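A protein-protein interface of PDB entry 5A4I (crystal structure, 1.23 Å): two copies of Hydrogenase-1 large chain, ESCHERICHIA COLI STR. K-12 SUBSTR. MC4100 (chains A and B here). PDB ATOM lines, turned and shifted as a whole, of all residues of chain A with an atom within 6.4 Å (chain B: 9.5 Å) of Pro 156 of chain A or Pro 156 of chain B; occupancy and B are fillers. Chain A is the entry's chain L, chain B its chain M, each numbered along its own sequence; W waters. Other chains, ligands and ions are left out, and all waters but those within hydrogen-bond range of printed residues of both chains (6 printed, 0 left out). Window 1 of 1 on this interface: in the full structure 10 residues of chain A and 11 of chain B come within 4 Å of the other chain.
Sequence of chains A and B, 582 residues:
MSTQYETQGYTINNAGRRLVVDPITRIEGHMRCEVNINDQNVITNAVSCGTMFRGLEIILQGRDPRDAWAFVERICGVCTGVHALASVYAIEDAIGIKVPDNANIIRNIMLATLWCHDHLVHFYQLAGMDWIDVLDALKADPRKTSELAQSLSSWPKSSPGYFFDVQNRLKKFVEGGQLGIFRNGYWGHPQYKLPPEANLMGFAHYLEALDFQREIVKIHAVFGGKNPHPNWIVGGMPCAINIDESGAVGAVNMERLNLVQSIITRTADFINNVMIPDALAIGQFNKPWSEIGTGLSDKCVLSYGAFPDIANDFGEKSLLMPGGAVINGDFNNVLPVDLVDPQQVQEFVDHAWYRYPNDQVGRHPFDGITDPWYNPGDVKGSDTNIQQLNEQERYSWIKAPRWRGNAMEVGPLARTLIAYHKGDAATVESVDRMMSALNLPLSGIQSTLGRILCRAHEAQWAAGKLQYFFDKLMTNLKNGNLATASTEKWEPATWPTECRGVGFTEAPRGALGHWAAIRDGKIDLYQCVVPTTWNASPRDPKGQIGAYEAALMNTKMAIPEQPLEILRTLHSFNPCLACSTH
The side-chain hydroxyl (OG) of Ser 153 of chain B is in hydrogen-bond range of the backbone NH (N) of Trp 155 of chain B (2.9 Å). OG of Ser 158 of chain B lies within hydrogen-bond range of O of Pro 156 of chain B (3.4 Å).
Pro 156 of chain B touches five residues of chain A. Of chain B, only Ser 159 comes within 4 Å of Trp 155 of chain A. Ser 158 of chain A touches just these residues of chain B: Pro 156 and Ser 159. Of the printed residues of chain A, Lys 157 of chain B touches Pro 156 and Lys 157. Asp 165 of chain B touches none of the printed residues of chain A. The nearest printed residue of chain A that does not touch Pro 156 of chain B is Gly 161 of chain A (6.3 Å).
Of the 24 printed residues of chain B, 11 touch a printed residue of chain A. Along chain B the printed residues that touch a printed residue of chain A span positions 146 to 162. Hydrophobic or aromatic side chains of chain A that line the printed part of chain B: Pro 156 and Tyr 162. Along chain A the printed residues that touch a printed residue of chain B span positions 150 to 162. Among the printed residues, no Asp or Glu carboxylate lies within 4 Å of a Lys or Arg side-chain nitrogen of the other chain.
Gln 150 of chain A touches its own counterpart, Gln 150 of chain B. Pro 156 of chain A touches Ser 159 of chain B, and with the chains exchanged Ser 159 of chain A touches Pro 156 of chain B.
Water W3 lies within hydrogen-bond range of the side-chain amide oxygen (OE1) of Gln 150 of chain B (3.0 Å) and the side-chain amide nitrogen (NE2) of Gln 150 of chain A (3.3 Å).
NE2 of Gln 150 of chain B is in hydrogen-bond range of OE1 of Gln 150 of chain A (2.9 Å). The backbone carbonyl oxygen of Trp 155 of chain A is in hydrogen-bond range of the side-chain hydroxyl of Ser 159 of chain B. N of Ser 158 of chain B is in hydrogen-bond range of O of Pro 156 of chain A, at 3.0 Å. The backbone carbonyl oxygen (O) of Pro 156 of chain A sits at hydrogen-bond distance from the backbone NH (N) of Ser 159 of chain B, 3.3 Å away. O of Pro 156 of chain B is in hydrogen-bond range of N of Ser 158 of chain A. N of Ser 159 of chain A lies within hydrogen-bond range of O of Pro 156 of chain B.
Gln 150 of chain A touches Ser 146 of chain B. Gln 150 of chain A touches Pro 160 of chain B (CD to CD, 3.4 Å). Tyr 162 of chain B touches Pro 156 of chain A. NE2 of Gln 150 of chain B touches CA of Ser 159 of chain A, at 3.7 Å.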
ATOM      1  N   GLN A 150      -9.042  -9.825   6.198  1.00  0.00           N
ATOM      2  CA  GLN A 150      -9.871 -10.484   7.178  1.00  0.00           C
ATOM      3  C   GLN A 150     -11.341 -10.135   7.060  1.00  0.00           C
ATOM      4  O   GLN A 150     -12.160 -10.922   7.444  1.00  0.00           O
ATOM      5  CB  GLN A 150      -9.346 -10.154   8.567  1.00  0.00           C
ATOM      6  CG  GLN A 150      -7.975 -10.802   8.758  1.00  0.00           C
ATOM      7  CD  GLN A 150      -7.231 -10.560  10.057  1.00  0.00           C
ATOM      8  OE1 GLN A 150      -6.141 -11.116  10.266  1.00  0.00           O
ATOM      9  NE2 GLN A 150      -7.768  -9.767  10.922  1.00  0.00           N
ATOM     10  N   SER A 153     -12.489 -12.637   3.945  1.00  0.00           N
ATOM     11  CA  SER A 153     -12.296 -14.072   3.885  1.00  0.00           C
ATOM     12  C   SER A 153     -11.878 -14.657   5.214  1.00  0.00           C
ATOM     13  O   SER A 153     -11.206 -13.973   5.990  1.00  0.00           O
ATOM     14  CB  SER A 153     -11.173 -14.398   2.855  1.00  0.00           C
ATOM     15  OG  SER A 153     -10.935 -15.781   2.812  1.00  0.00           O
ATOM     16  N   SER A 154     -12.151 -15.945   5.373  1.00  0.00           N
ATOM     17  CA  SER A 154     -11.610 -16.708   6.504  1.00  0.00           C
ATOM     18  C   SER A 154     -10.189 -17.249   6.262  1.00  0.00           C
ATOM     19  O   SER A 154      -9.606 -17.913   7.121  1.00  0.00           O
ATOM     20  CB  SER A 154     -12.508 -17.868   6.830  1.00  0.00           C
ATOM     21  OG  SER A 154     -12.663 -18.711   5.703  1.00  0.00           O
ATOM     22  N   TRP A 155      -9.653 -17.057   5.053  1.00  0.00           N
ATOM     23  CA  TRP A 155      -8.337 -17.594   4.719  1.00  0.00           C
ATOM     24  C   TRP A 155      -7.357 -17.321   5.843  1.00  0.00           C
ATOM     25  O   TRP A 155      -7.269 -16.215   6.326  1.00  0.00           O
ATOM     26  CB  TRP A 155      -7.821 -16.972   3.435  1.00  0.00           C
ATOM     27  CG  TRP A 155      -6.574 -17.564   2.884  1.00  0.00           C
ATOM     28  CD1 TRP A 155      -5.452 -16.891   2.583  1.00  0.00           C
ATOM     29  CD2 TRP A 155      -6.381 -18.908   2.426  1.00  0.00           C
ATOM     30  NE1 TRP A 155      -4.538 -17.743   2.003  1.00  0.00           N
ATOM     31  CE2 TRP A 155      -5.087 -18.980   1.909  1.00  0.00           C
ATOM     32  CE3 TRP A 155      -7.160 -20.060   2.429  1.00  0.00           C
ATOM     33  CZ2 TRP A 155      -4.553 -20.166   1.385  1.00  0.00           C
ATOM     34  CZ3 TRP A 155      -6.622 -21.238   1.889  1.00  0.00           C
ATOM     35  CH2 TRP A 155      -5.354 -21.256   1.385  1.00  0.00           C
ATOM     36  N   PRO A 156      -6.533 -18.304   6.226  1.00  0.00           N
ATOM     37  CA  PRO A 156      -5.671 -18.045   7.410  1.00  0.00           C
ATOM     38  C   PRO A 156      -4.616 -16.996   7.233  1.00  0.00           C
ATOM     39  O   PRO A 156      -4.291 -16.286   8.196  1.00  0.00           O
ATOM     40  CB  PRO A 156      -5.058 -19.416   7.688  1.00  0.00           C
ATOM     41  CG  PRO A 156      -6.062 -20.380   7.178  1.00  0.00           C
ATOM     42  CD  PRO A 156      -6.599 -19.737   5.927  1.00  0.00           C
ATOM     43  N   LYS A 157      -4.046 -16.877   6.043  1.00  0.00           N
ATOM     44  CA  LYS A 157      -2.809 -16.134   5.858  1.00  0.00           C
ATOM     45  C   LYS A 157      -3.084 -14.656   5.668  1.00  0.00           C
ATOM     46  O   LYS A 157      -3.265 -14.169   4.553  1.00  0.00           O
ATOM     47  CB  LYS A 157      -2.054 -16.708   4.672  1.00  0.00           C
ATOM     48  CG  LYS A 157      -1.620 -18.135   4.870  1.00  0.00           C
ATOM     49  CD  LYS A 157      -0.714 -18.536   3.682  1.00  0.00           C
ATOM     50  CE  LYS A 157      -0.262 -19.958   3.854  1.00  0.00           C
ATOM     51  NZ  LYS A 157       0.625 -20.249   2.717  1.00  0.00           N
ATOM     52  N   SER A 158      -3.161 -13.930   6.778  1.00  0.00           N
ATOM     53  CA  SER A 158      -3.645 -12.562   6.761  1.00  0.00           C
ATOM     54  C   SER A 158      -2.961 -11.685   7.781  1.00  0.00           C
ATOM     55  O   SER A 158      -3.377 -10.563   7.972  1.00  0.00           O
ATOM     56  CB  SER A 158      -5.178 -12.539   7.045  1.00  0.00           C
ATOM     57  OG  SER A 158      -5.353 -12.986   8.398  1.00  0.00           O
ATOM     58  N   SER A 159      -1.872 -12.137   8.417  1.00  0.00           N
ATOM     59  CA  SER A 159      -1.333 -11.356   9.516  1.00  0.00           C
ATOM     60  C   SER A 159      -0.685 -10.068   8.960  1.00  0.00           C
ATOM     61  O   SER A 159      -0.166 -10.026   7.833  1.00  0.00           O
ATOM     62  CB  SER A 159      -0.306 -12.159  10.304  1.00  0.00           C
ATOM     63  OG  SER A 159       0.913 -12.275   9.596  1.00  0.00           O
ATOM     64  N   GLY A 161       2.183  -9.009   9.840  1.00  0.00           N
ATOM     65  CA  GLY A 161       3.591  -9.336   9.610  1.00  0.00           C
ATOM     66  C   GLY A 161       3.788 -10.050   8.280  1.00  0.00           C
ATOM     67  O   GLY A 161       4.803  -9.824   7.611  1.00  0.00           O
ATOM     68  N   TYR A 162       2.837 -10.881   7.889  1.00  0.00           N
ATOM     69  CA  TYR A 162       2.874 -11.513   6.578  1.00  0.00           C
ATOM     70  C   TYR A 162       2.821 -10.488   5.471  1.00  0.00           C
ATOM     71  O   TYR A 162       3.649 -10.492   4.552  1.00  0.00           O
ATOM     72  CB  TYR A 162       1.704 -12.476   6.446  1.00  0.00           C
ATOM     73  CG  TYR A 162       1.470 -13.053   5.067  1.00  0.00           C
ATOM     74  CD1 TYR A 162       2.462 -13.773   4.379  1.00  0.00           C
ATOM     75  CD2 TYR A 162       0.230 -12.922   4.458  1.00  0.00           C
ATOM     76  CE1 TYR A 162       2.190 -14.288   3.130  1.00  0.00           C
ATOM     77  CE2 TYR A 162      -0.018 -13.458   3.201  1.00  0.00           C
ATOM     78  CZ  TYR A 162       0.968 -14.127   2.553  1.00  0.00           C
ATOM     79  OH  TYR A 162       0.727 -14.676   1.306  1.00  0.00           O
ATOM     80  N   ASP A 165       6.016  -8.638   5.323  1.00  0.00           N
ATOM     81  CA  ASP A 165       7.081  -9.478   4.737  1.00  0.00           C
ATOM     82  C   ASP A 165       6.953  -9.537   3.194  1.00  0.00           C
ATOM     83  O   ASP A 165       7.933  -9.384   2.476  1.00  0.00           O
ATOM     84  CB  ASP A 165       7.032 -10.885   5.338  1.00  0.00           C
ATOM     85  CG  ASP A 165       7.522 -10.962   6.832  1.00  0.00           C
ATOM     86  OD1 ASP A 165       8.147  -9.995   7.319  1.00  0.00           O
ATOM     87  OD2 ASP A 165       7.293 -12.030   7.485  1.00  0.00           O
ATOM     88  N   ASP A 269     -10.353 -25.461  -1.089  1.00  0.00           N
ATOM     89  CA  ASP A 269     -10.086 -24.477  -0.014  1.00  0.00           C
ATOM     90  C   ASP A 269      -9.471 -23.215  -0.611  1.00  0.00           C
ATOM     91  O   ASP A 269      -9.860 -22.094  -0.312  1.00  0.00           O
ATOM     92  CB  ASP A 269      -9.161 -25.122   1.046  1.00  0.00           C
ATOM     93  CG  ASP A 269      -9.017 -24.305   2.360  1.00  0.00           C
ATOM     94  OD1 ASP A 269      -9.815 -23.406   2.679  1.00  0.00           O
ATOM     95  OD2 ASP A 269      -8.054 -24.604   3.067  1.00  0.00           O
ATOM     96  N   ASN A 273     -11.556 -19.620  -0.800  1.00  0.00           N
ATOM     97  CA  ASN A 273     -11.141 -18.624   0.186  1.00  0.00           C
ATOM     98  C   ASN A 273     -10.117 -17.608  -0.255  1.00  0.00           C
ATOM     99  O   ASN A 273      -9.886 -16.646   0.456  1.00  0.00           O
ATOM    100  CB  ASN A 273     -10.727 -19.348   1.477  1.00  0.00           C
ATOM    101  CG  ASN A 273     -11.880 -20.156   2.047  1.00  0.00           C
ATOM    102  OD1 ASN A 273     -12.872 -19.597   2.453  1.00  0.00           O
ATOM    103  ND2 ASN A 273     -11.808 -21.480   1.958  1.00  0.00           N
ATOM    104  N   SER B 146      -6.858 -14.048  17.249  1.00  0.00           N
ATOM    105  CA  SER B 146      -6.133 -13.412  16.143  1.00  0.00           C
ATOM    106  C   SER B 146      -5.271 -12.257  16.621  1.00  0.00           C
ATOM    107  O   SER B 146      -4.092 -12.139  16.270  1.00  0.00           O
ATOM    108  CB  SER B 146      -7.094 -12.938  15.090  1.00  0.00           C
ATOM    109  OG  SER B 146      -6.457 -12.255  14.062  1.00  0.00           O
ATOM    110  N   ALA B 149      -2.259 -13.591  18.638  1.00  0.00           N
ATOM    111  CA  ALA B 149      -1.268 -14.240  17.746  1.00  0.00           C
ATOM    112  C   ALA B 149      -0.460 -13.181  16.985  1.00  0.00           C
ATOM    113  O   ALA B 149       0.792 -13.232  16.900  1.00  0.00           O
ATOM    114  CB  ALA B 149      -1.996 -15.213  16.814  1.00  0.00           C
ATOM    115  N   GLN B 150      -1.156 -12.194  16.440  1.00  0.00           N
ATOM    116  CA  GLN B 150      -0.530 -11.148  15.642  1.00  0.00           C
ATOM    117  C   GLN B 150       0.360 -10.231  16.466  1.00  0.00           C
ATOM    118  O   GLN B 150       1.341  -9.679  15.960  1.00  0.00           O
ATOM    119  CB  GLN B 150      -1.611 -10.383  14.897  1.00  0.00           C
ATOM    120  CG  GLN B 150      -2.266 -11.259  13.840  1.00  0.00           C
ATOM    121  CD  GLN B 150      -3.409 -10.593  13.080  1.00  0.00           C
ATOM    122  OE1 GLN B 150      -3.808  -9.465  13.369  1.00  0.00           O
ATOM    123  NE2 GLN B 150      -3.936 -11.280  12.125  1.00  0.00           N
ATOM    124  N   SER B 153       3.744 -12.569  16.774  1.00  0.00           N
ATOM    125  CA  SER B 153       4.442 -13.180  15.641  1.00  0.00           C
ATOM    126  C   SER B 153       3.992 -12.633  14.345  1.00  0.00           C
ATOM    127  O   SER B 153       2.842 -12.185  14.195  1.00  0.00           O
ATOM    128  CB  SER B 153       4.167 -14.686  15.668  1.00  0.00           C
ATOM    129  OG  SER B 153       4.823 -15.329  14.585  1.00  0.00           O
ATOM    130  N   SER B 154       4.910 -12.711  13.378  1.00  0.00           N
ATOM    131  CA  SER B 154       4.620 -12.416  11.986  1.00  0.00           C
ATOM    132  C   SER B 154       4.048 -13.615  11.223  1.00  0.00           C
ATOM    133  O   SER B 154       3.694 -13.486  10.050  1.00  0.00           O
ATOM    134  CB  SER B 154       5.895 -11.921  11.288  1.00  0.00           C
ATOM    135  OG  SER B 154       6.927 -12.884  11.424  1.00  0.00           O
ATOM    136  N   TRP B 155       3.914 -14.763  11.883  1.00  0.00           N
ATOM    137  CA  TRP B 155       3.421 -15.963  11.221  1.00  0.00           C
ATOM    138  C   TRP B 155       2.158 -15.639  10.440  1.00  0.00           C
ATOM    139  O   TRP B 155       1.260 -14.980  10.960  1.00  0.00           O
ATOM    140  CB  TRP B 155       3.116 -17.048  12.242  1.00  0.00           C
ATOM    141  CG  TRP B 155       2.735 -18.376  11.684  1.00  0.00           C
ATOM    142  CD1 TRP B 155       1.628 -19.076  11.969  1.00  0.00           C
ATOM    143  CD2 TRP B 155       3.549 -19.222  10.822  1.00  0.00           C
ATOM    144  NE1 TRP B 155       1.677 -20.306  11.326  1.00  0.00           N
ATOM    145  CE2 TRP B 155       2.858 -20.417  10.656  1.00  0.00           C
ATOM    146  CE3 TRP B 155       4.822 -19.096  10.261  1.00  0.00           C
ATOM    147  CZ2 TRP B 155       3.362 -21.472   9.891  1.00  0.00           C
ATOM    148  CZ3 TRP B 155       5.336 -20.167   9.513  1.00  0.00           C
ATOM    149  CH2 TRP B 155       4.601 -21.312   9.352  1.00  0.00           C
ATOM    150  N   PRO B 156       2.028 -16.108   9.192  1.00  0.00           N
ATOM    151  CA  PRO B 156       0.845 -15.648   8.438  1.00  0.00           C
ATOM    152  C   PRO B 156      -0.495 -16.110   8.957  1.00  0.00           C
ATOM    153  O   PRO B 156      -1.467 -15.380   8.810  1.00  0.00           O
ATOM    154  CB  PRO B 156       1.108 -16.201   7.042  1.00  0.00           C
ATOM    155  CG  PRO B 156       2.609 -16.251   6.930  1.00  0.00           C
ATOM    156  CD  PRO B 156       3.040 -16.722   8.295  1.00  0.00           C
ATOM    157  N   LYS B 157      -0.585 -17.330   9.492  1.00  0.00           N
ATOM    158  CA  LYS B 157      -1.845 -18.035   9.743  1.00  0.00           C
ATOM    159  C   LYS B 157      -2.436 -17.591  11.055  1.00  0.00           C
ATOM    160  O   LYS B 157      -2.223 -18.215  12.089  1.00  0.00           O
ATOM    161  CB  LYS B 157      -1.671 -19.564   9.699  1.00  0.00           C
ATOM    162  CG  LYS B 157      -1.185 -20.030   8.350  1.00  0.00           C
ATOM    163  CD  LYS B 157      -1.149 -21.547   8.366  1.00  0.00           C
ATOM    164  CE  LYS B 157      -0.663 -22.116   7.070  1.00  0.00           C
ATOM    165  NZ  LYS B 157      -0.679 -23.598   7.241  1.00  0.00           N
ATOM    166  N   SER B 158      -3.215 -16.517  10.993  1.00  0.00           N
ATOM    167  CA  SER B 158      -3.681 -15.873  12.186  1.00  0.00           C
ATOM    168  C   SER B 158      -5.032 -15.234  12.044  1.00  0.00           C
ATOM    169  O   SER B 158      -5.416 -14.489  12.960  1.00  0.00           O
ATOM    170  CB  SER B 158      -2.673 -14.785  12.614  1.00  0.00           C
ATOM    171  OG  SER B 158      -2.687 -13.814  11.596  1.00  0.00           O
ATOM    172  N   SER B 159      -5.775 -15.459  10.971  1.00  0.00           N
ATOM    173  CA  SER B 159      -7.028 -14.730  10.768  1.00  0.00           C
ATOM    174  C   SER B 159      -8.062 -15.161  11.806  1.00  0.00           C
ATOM    175  O   SER B 159      -8.054 -16.273  12.307  1.00  0.00           O
ATOM    176  CB  SER B 159      -7.591 -14.986   9.366  1.00  0.00           C
ATOM    177  OG  SER B 159      -8.155 -16.259   9.267  1.00  0.00           O
ATOM    178  N   PRO B 160      -9.009 -14.257  12.128  1.00  0.00           N
ATOM    179  CA  PRO B 160     -10.085 -14.662  13.033  1.00  0.00           C
ATOM    180  C   PRO B 160     -10.868 -15.876  12.473  1.00  0.00           C
ATOM    181  O   PRO B 160     -11.266 -16.792  13.227  1.00  0.00           O
ATOM    182  CB  PRO B 160     -10.978 -13.391  13.079  1.00  0.00           C
ATOM    183  CG  PRO B 160     -10.013 -12.286  12.845  1.00  0.00           C
ATOM    184  CD  PRO B 160      -9.033 -12.828  11.822  1.00  0.00           C
ATOM    185  N   GLY B 161     -11.059 -15.912  11.145  1.00  0.00           N
ATOM    186  CA  GLY B 161     -11.753 -17.039  10.549  1.00  0.00           C
ATOM    187  C   GLY B 161     -11.019 -18.374  10.711  1.00  0.00           C
ATOM    188  O   GLY B 161     -11.648 -19.397  10.881  1.00  0.00           O
ATOM    189  N   TYR B 162      -9.697 -18.344  10.625  1.00  0.00           N
ATOM    190  CA  TYR B 162      -8.894 -19.512  10.897  1.00  0.00           C
ATOM    191  C   TYR B 162      -9.106 -20.014  12.306  1.00  0.00           C
ATOM    192  O   TYR B 162      -9.370 -21.187  12.516  1.00  0.00           O
ATOM    193  CB  TYR B 162      -7.438 -19.177  10.625  1.00  0.00           C
ATOM    194  CG  TYR B 162      -6.446 -20.219  11.070  1.00  0.00           C
ATOM    195  CD1 TYR B 162      -6.504 -21.520  10.584  1.00  0.00           C
ATOM    196  CD2 TYR B 162      -5.476 -19.923  12.003  1.00  0.00           C
ATOM    197  CE1 TYR B 162      -5.571 -22.444  10.968  1.00  0.00           C
ATOM    198  CE2 TYR B 162      -4.545 -20.876  12.404  1.00  0.00           C
ATOM    199  CZ  TYR B 162      -4.614 -22.119  11.869  1.00  0.00           C
ATOM    200  OH  TYR B 162      -3.717 -23.040  12.282  1.00  0.00           O
ATOM    201  N   PHE B 163      -8.993 -19.129  13.278  1.00  0.00           N
ATOM    202  CA  PHE B 163      -9.158 -19.566  14.674  1.00  0.00           C
ATOM    203  C   PHE B 163     -10.577 -20.024  14.915  1.00  0.00           C
ATOM    204  O   PHE B 163     -10.806 -21.007  15.646  1.00  0.00           O
ATOM    205  CB  PHE B 163      -8.706 -18.483  15.638  1.00  0.00           C
ATOM    206  CG  PHE B 163      -7.205 -18.296  15.651  1.00  0.00           C
ATOM    207  CD1 PHE B 163      -6.379 -19.366  15.996  1.00  0.00           C
ATOM    208  CD2 PHE B 163      -6.576 -17.110  15.248  1.00  0.00           C
ATOM    209  CE1 PHE B 163      -5.002 -19.226  16.014  1.00  0.00           C
ATOM    210  CE2 PHE B 163      -5.203 -16.960  15.303  1.00  0.00           C
ATOM    211  CZ  PHE B 163      -4.402 -18.032  15.667  1.00  0.00           C
ATOM    212  N   PHE B 164     -11.559 -19.380  14.270  1.00  0.00           N
ATOM    213  CA  PHE B 164     -12.933 -19.890  14.386  1.00  0.00           C
ATOM    214  C   PHE B 164     -13.066 -21.291  13.819  1.00  0.00           C
ATOM    215  O   PHE B 164     -13.711 -22.161  14.402  1.00  0.00           O
ATOM    216  CB  PHE B 164     -13.885 -18.898  13.710  1.00  0.00           C
ATOM    217  CG  PHE B 164     -15.346 -19.209  13.899  1.00  0.00           C
ATOM    218  CD1 PHE B 164     -15.880 -19.371  15.174  1.00  0.00           C
ATOM    219  CD2 PHE B 164     -16.190 -19.333  12.805  1.00  0.00           C
ATOM    220  CE1 PHE B 164     -17.231 -19.664  15.359  1.00  0.00           C
ATOM    221  CE2 PHE B 164     -17.562 -19.598  12.975  1.00  0.00           C
ATOM    222  CZ  PHE B 164     -18.071 -19.763  14.252  1.00  0.00           C
ATOM    223  N   ASP B 165     -12.478 -21.500  12.655  1.00  0.00           N
ATOM    224  CA  ASP B 165     -12.493 -22.838  12.019  1.00  0.00           C
ATOM    225  C   ASP B 165     -11.817 -23.921  12.907  1.00  0.00           C
ATOM    226  O   ASP B 165     -12.344 -25.032  13.063  1.00  0.00           O
ATOM    227  CB  ASP B 165     -11.818 -22.806  10.619  1.00  0.00           C
ATOM    228  CG  ASP B 165     -12.635 -22.026   9.541  1.00  0.00           C
ATOM    229  OD1 ASP B 165     -13.842 -21.724   9.720  1.00  0.00           O
ATOM    230  OD2 ASP B 165     -12.051 -21.718   8.467  1.00  0.00           O
ATOM    231  N   VAL B 166     -10.702 -23.582  13.509  1.00  0.00           N
ATOM    232  CA  VAL B 166     -10.027 -24.530  14.396  1.00  0.00           C
ATOM    233  C   VAL B 166     -10.922 -24.840  15.614  1.00  0.00           C
ATOM    234  O   VAL B 166     -11.163 -25.986  15.983  1.00  0.00           O
ATOM    235  CB  VAL B 166      -8.646 -23.983  14.853  1.00  0.00           C
ATOM    236  CG1 VAL B 166      -8.065 -24.820  15.987  1.00  0.00           C
ATOM    237  CG2 VAL B 166      -7.667 -23.891  13.683  1.00  0.00           C
ATOM    238  N   ALA B 204      -4.296 -24.488  17.941  1.00  0.00           N
ATOM    239  CA  ALA B 204      -4.101 -24.342  16.512  1.00  0.00           C
ATOM    240  C   ALA B 204      -2.660 -24.716  16.139  1.00  0.00           C
ATOM    241  O   ALA B 204      -2.445 -25.418  15.123  1.00  0.00           O
ATOM    242  CB  ALA B 204      -4.396 -22.930  16.066  1.00  0.00           C
ATOM    243  N   HIS B 205      -1.699 -24.224  16.907  1.00  0.00           N
ATOM    244  CA  HIS B 205      -0.315 -24.534  16.608  1.00  0.00           C
ATOM    245  C   HIS B 205       0.061 -25.981  16.831  1.00  0.00           C
ATOM    246  O   HIS B 205       0.885 -26.498  16.078  1.00  0.00           O
ATOM    247  CB  HIS B 205       0.609 -23.574  17.339  1.00  0.00           C
ATOM    248  CG  HIS B 205       0.409 -22.148  16.907  1.00  0.00           C
ATOM    249  ND1 HIS B 205       0.943 -21.084  17.596  1.00  0.00           N
ATOM    250  CD2 HIS B 205      -0.241 -21.618  15.834  1.00  0.00           C
ATOM    251  CE1 HIS B 205       0.645 -19.961  16.970  1.00  0.00           C
ATOM    252  NE2 HIS B 205      -0.074 -20.256  15.896  1.00  0.00           N
ATOM    253  N   GLU B 208      -0.924 -27.439  13.605  1.00  0.00           N
ATOM    254  CA  GLU B 208       0.010 -27.035  12.531  1.00  0.00           C
ATOM    255  C   GLU B 208       1.319 -27.808  12.654  1.00  0.00           C
ATOM    256  O   GLU B 208       1.929 -28.193  11.651  1.00  0.00           O
ATOM    257  CB  GLU B 208       0.297 -25.542  12.544  1.00  0.00           C
ATOM    258  CG  GLU B 208      -0.886 -24.676  12.122  1.00  0.00           C
ATOM    259  CD  GLU B 208      -0.524 -23.188  12.055  1.00  0.00           C
ATOM    260  OE1 GLU B 208       0.522 -22.884  11.467  1.00  0.00           O
ATOM    261  OE2 GLU B 208      -1.299 -22.336  12.581  1.00  0.00           O
ATOM    262  N   ASP B 269      11.587 -21.311   9.340  1.00  0.00           N
ATOM    263  CA  ASP B 269      10.435 -20.379   9.373  1.00  0.00           C
ATOM    264  C   ASP B 269       9.458 -20.839  10.456  1.00  0.00           C
ATOM    265  O   ASP B 269       8.939 -20.051  11.263  1.00  0.00           O
ATOM    266  CB  ASP B 269       9.723 -20.371   8.004  1.00  0.00           C
ATOM    267  CG  ASP B 269       8.632 -19.292   7.868  1.00  0.00           C
ATOM    268  OD1 ASP B 269       8.662 -18.242   8.527  1.00  0.00           O
ATOM    269  OD2 ASP B 269       7.724 -19.524   7.059  1.00  0.00           O
ATOM    270  N   PHE B 270       9.153 -22.127  10.470  1.00  0.00           N
ATOM    271  CA  PHE B 270       8.146 -22.651  11.416  1.00  0.00           C
ATOM    272  C   PHE B 270       8.654 -22.512  12.851  1.00  0.00           C
ATOM    273  O   PHE B 270       7.936 -22.075  13.772  1.00  0.00           O
ATOM    274  CB  PHE B 270       7.780 -24.108  11.062  1.00  0.00           C
ATOM    275  CG  PHE B 270       6.529 -24.583  11.757  1.00  0.00           C
ATOM    276  CD1 PHE B 270       6.562 -25.038  13.051  1.00  0.00           C
ATOM    277  CD2 PHE B 270       5.305 -24.540  11.097  1.00  0.00           C
ATOM    278  CE1 PHE B 270       5.395 -25.401  13.692  1.00  0.00           C
ATOM    279  CE2 PHE B 270       4.139 -24.979  11.698  1.00  0.00           C
ATOM    280  CZ  PHE B 270       4.171 -25.351  13.022  1.00  0.00           C
ATOM    281  N   ASN B 273       8.840 -18.700  13.980  1.00  0.00           N
ATOM    282  CA  ASN B 273       7.620 -17.894  13.964  1.00  0.00           C
ATOM    283  C   ASN B 273       6.427 -18.556  14.623  1.00  0.00           C
ATOM    284  O   ASN B 273       5.396 -17.895  14.834  1.00  0.00           O
ATOM    285  CB  ASN B 273       7.307 -17.411  12.562  1.00  0.00           C
ATOM    286  CG  ASN B 273       8.404 -16.550  12.046  1.00  0.00           C
ATOM    287  OD1 ASN B 273       8.625 -15.454  12.557  1.00  0.00           O
ATOM    288  ND2 ASN B 273       9.167 -17.062  11.094  1.00  0.00           N
ATOM    289  N   VAL B 274       6.528 -19.849  14.966  1.00  0.00           N
ATOM    290  CA  VAL B 274       5.448 -20.573  15.649  1.00  0.00           C
ATOM    291  C   VAL B 274       5.941 -21.039  17.012  1.00  0.00           C
ATOM    292  O   VAL B 274       5.414 -20.584  18.058  1.00  0.00           O
ATOM    293  CB  VAL B 274       4.906 -21.741  14.812  1.00  0.00           C
ATOM    294  CG1 VAL B 274       3.733 -22.421  15.512  1.00  0.00           C
ATOM    295  CG2 VAL B 274       4.503 -21.227  13.434  1.00  0.00           C
HETATM  296  O   HOH W   1     -10.834 -13.902   8.961  1.00  0.00           O
HETATM  297  O   HOH W   2       1.555 -10.177  12.505  1.00  0.00           O
HETATM  298  O   HOH W   3      -5.415  -7.546  11.706  1.00  0.00           O
HETATM  299  O   HOH W   4      -7.032  -9.559  13.790  1.00  0.00           O
HETATM  300  O   HOH W   5       5.241 -13.664   7.669  1.00  0.00           O
HETATM  301  O   HOH W   6      -9.744 -20.704   7.758  1.00  0.00           O
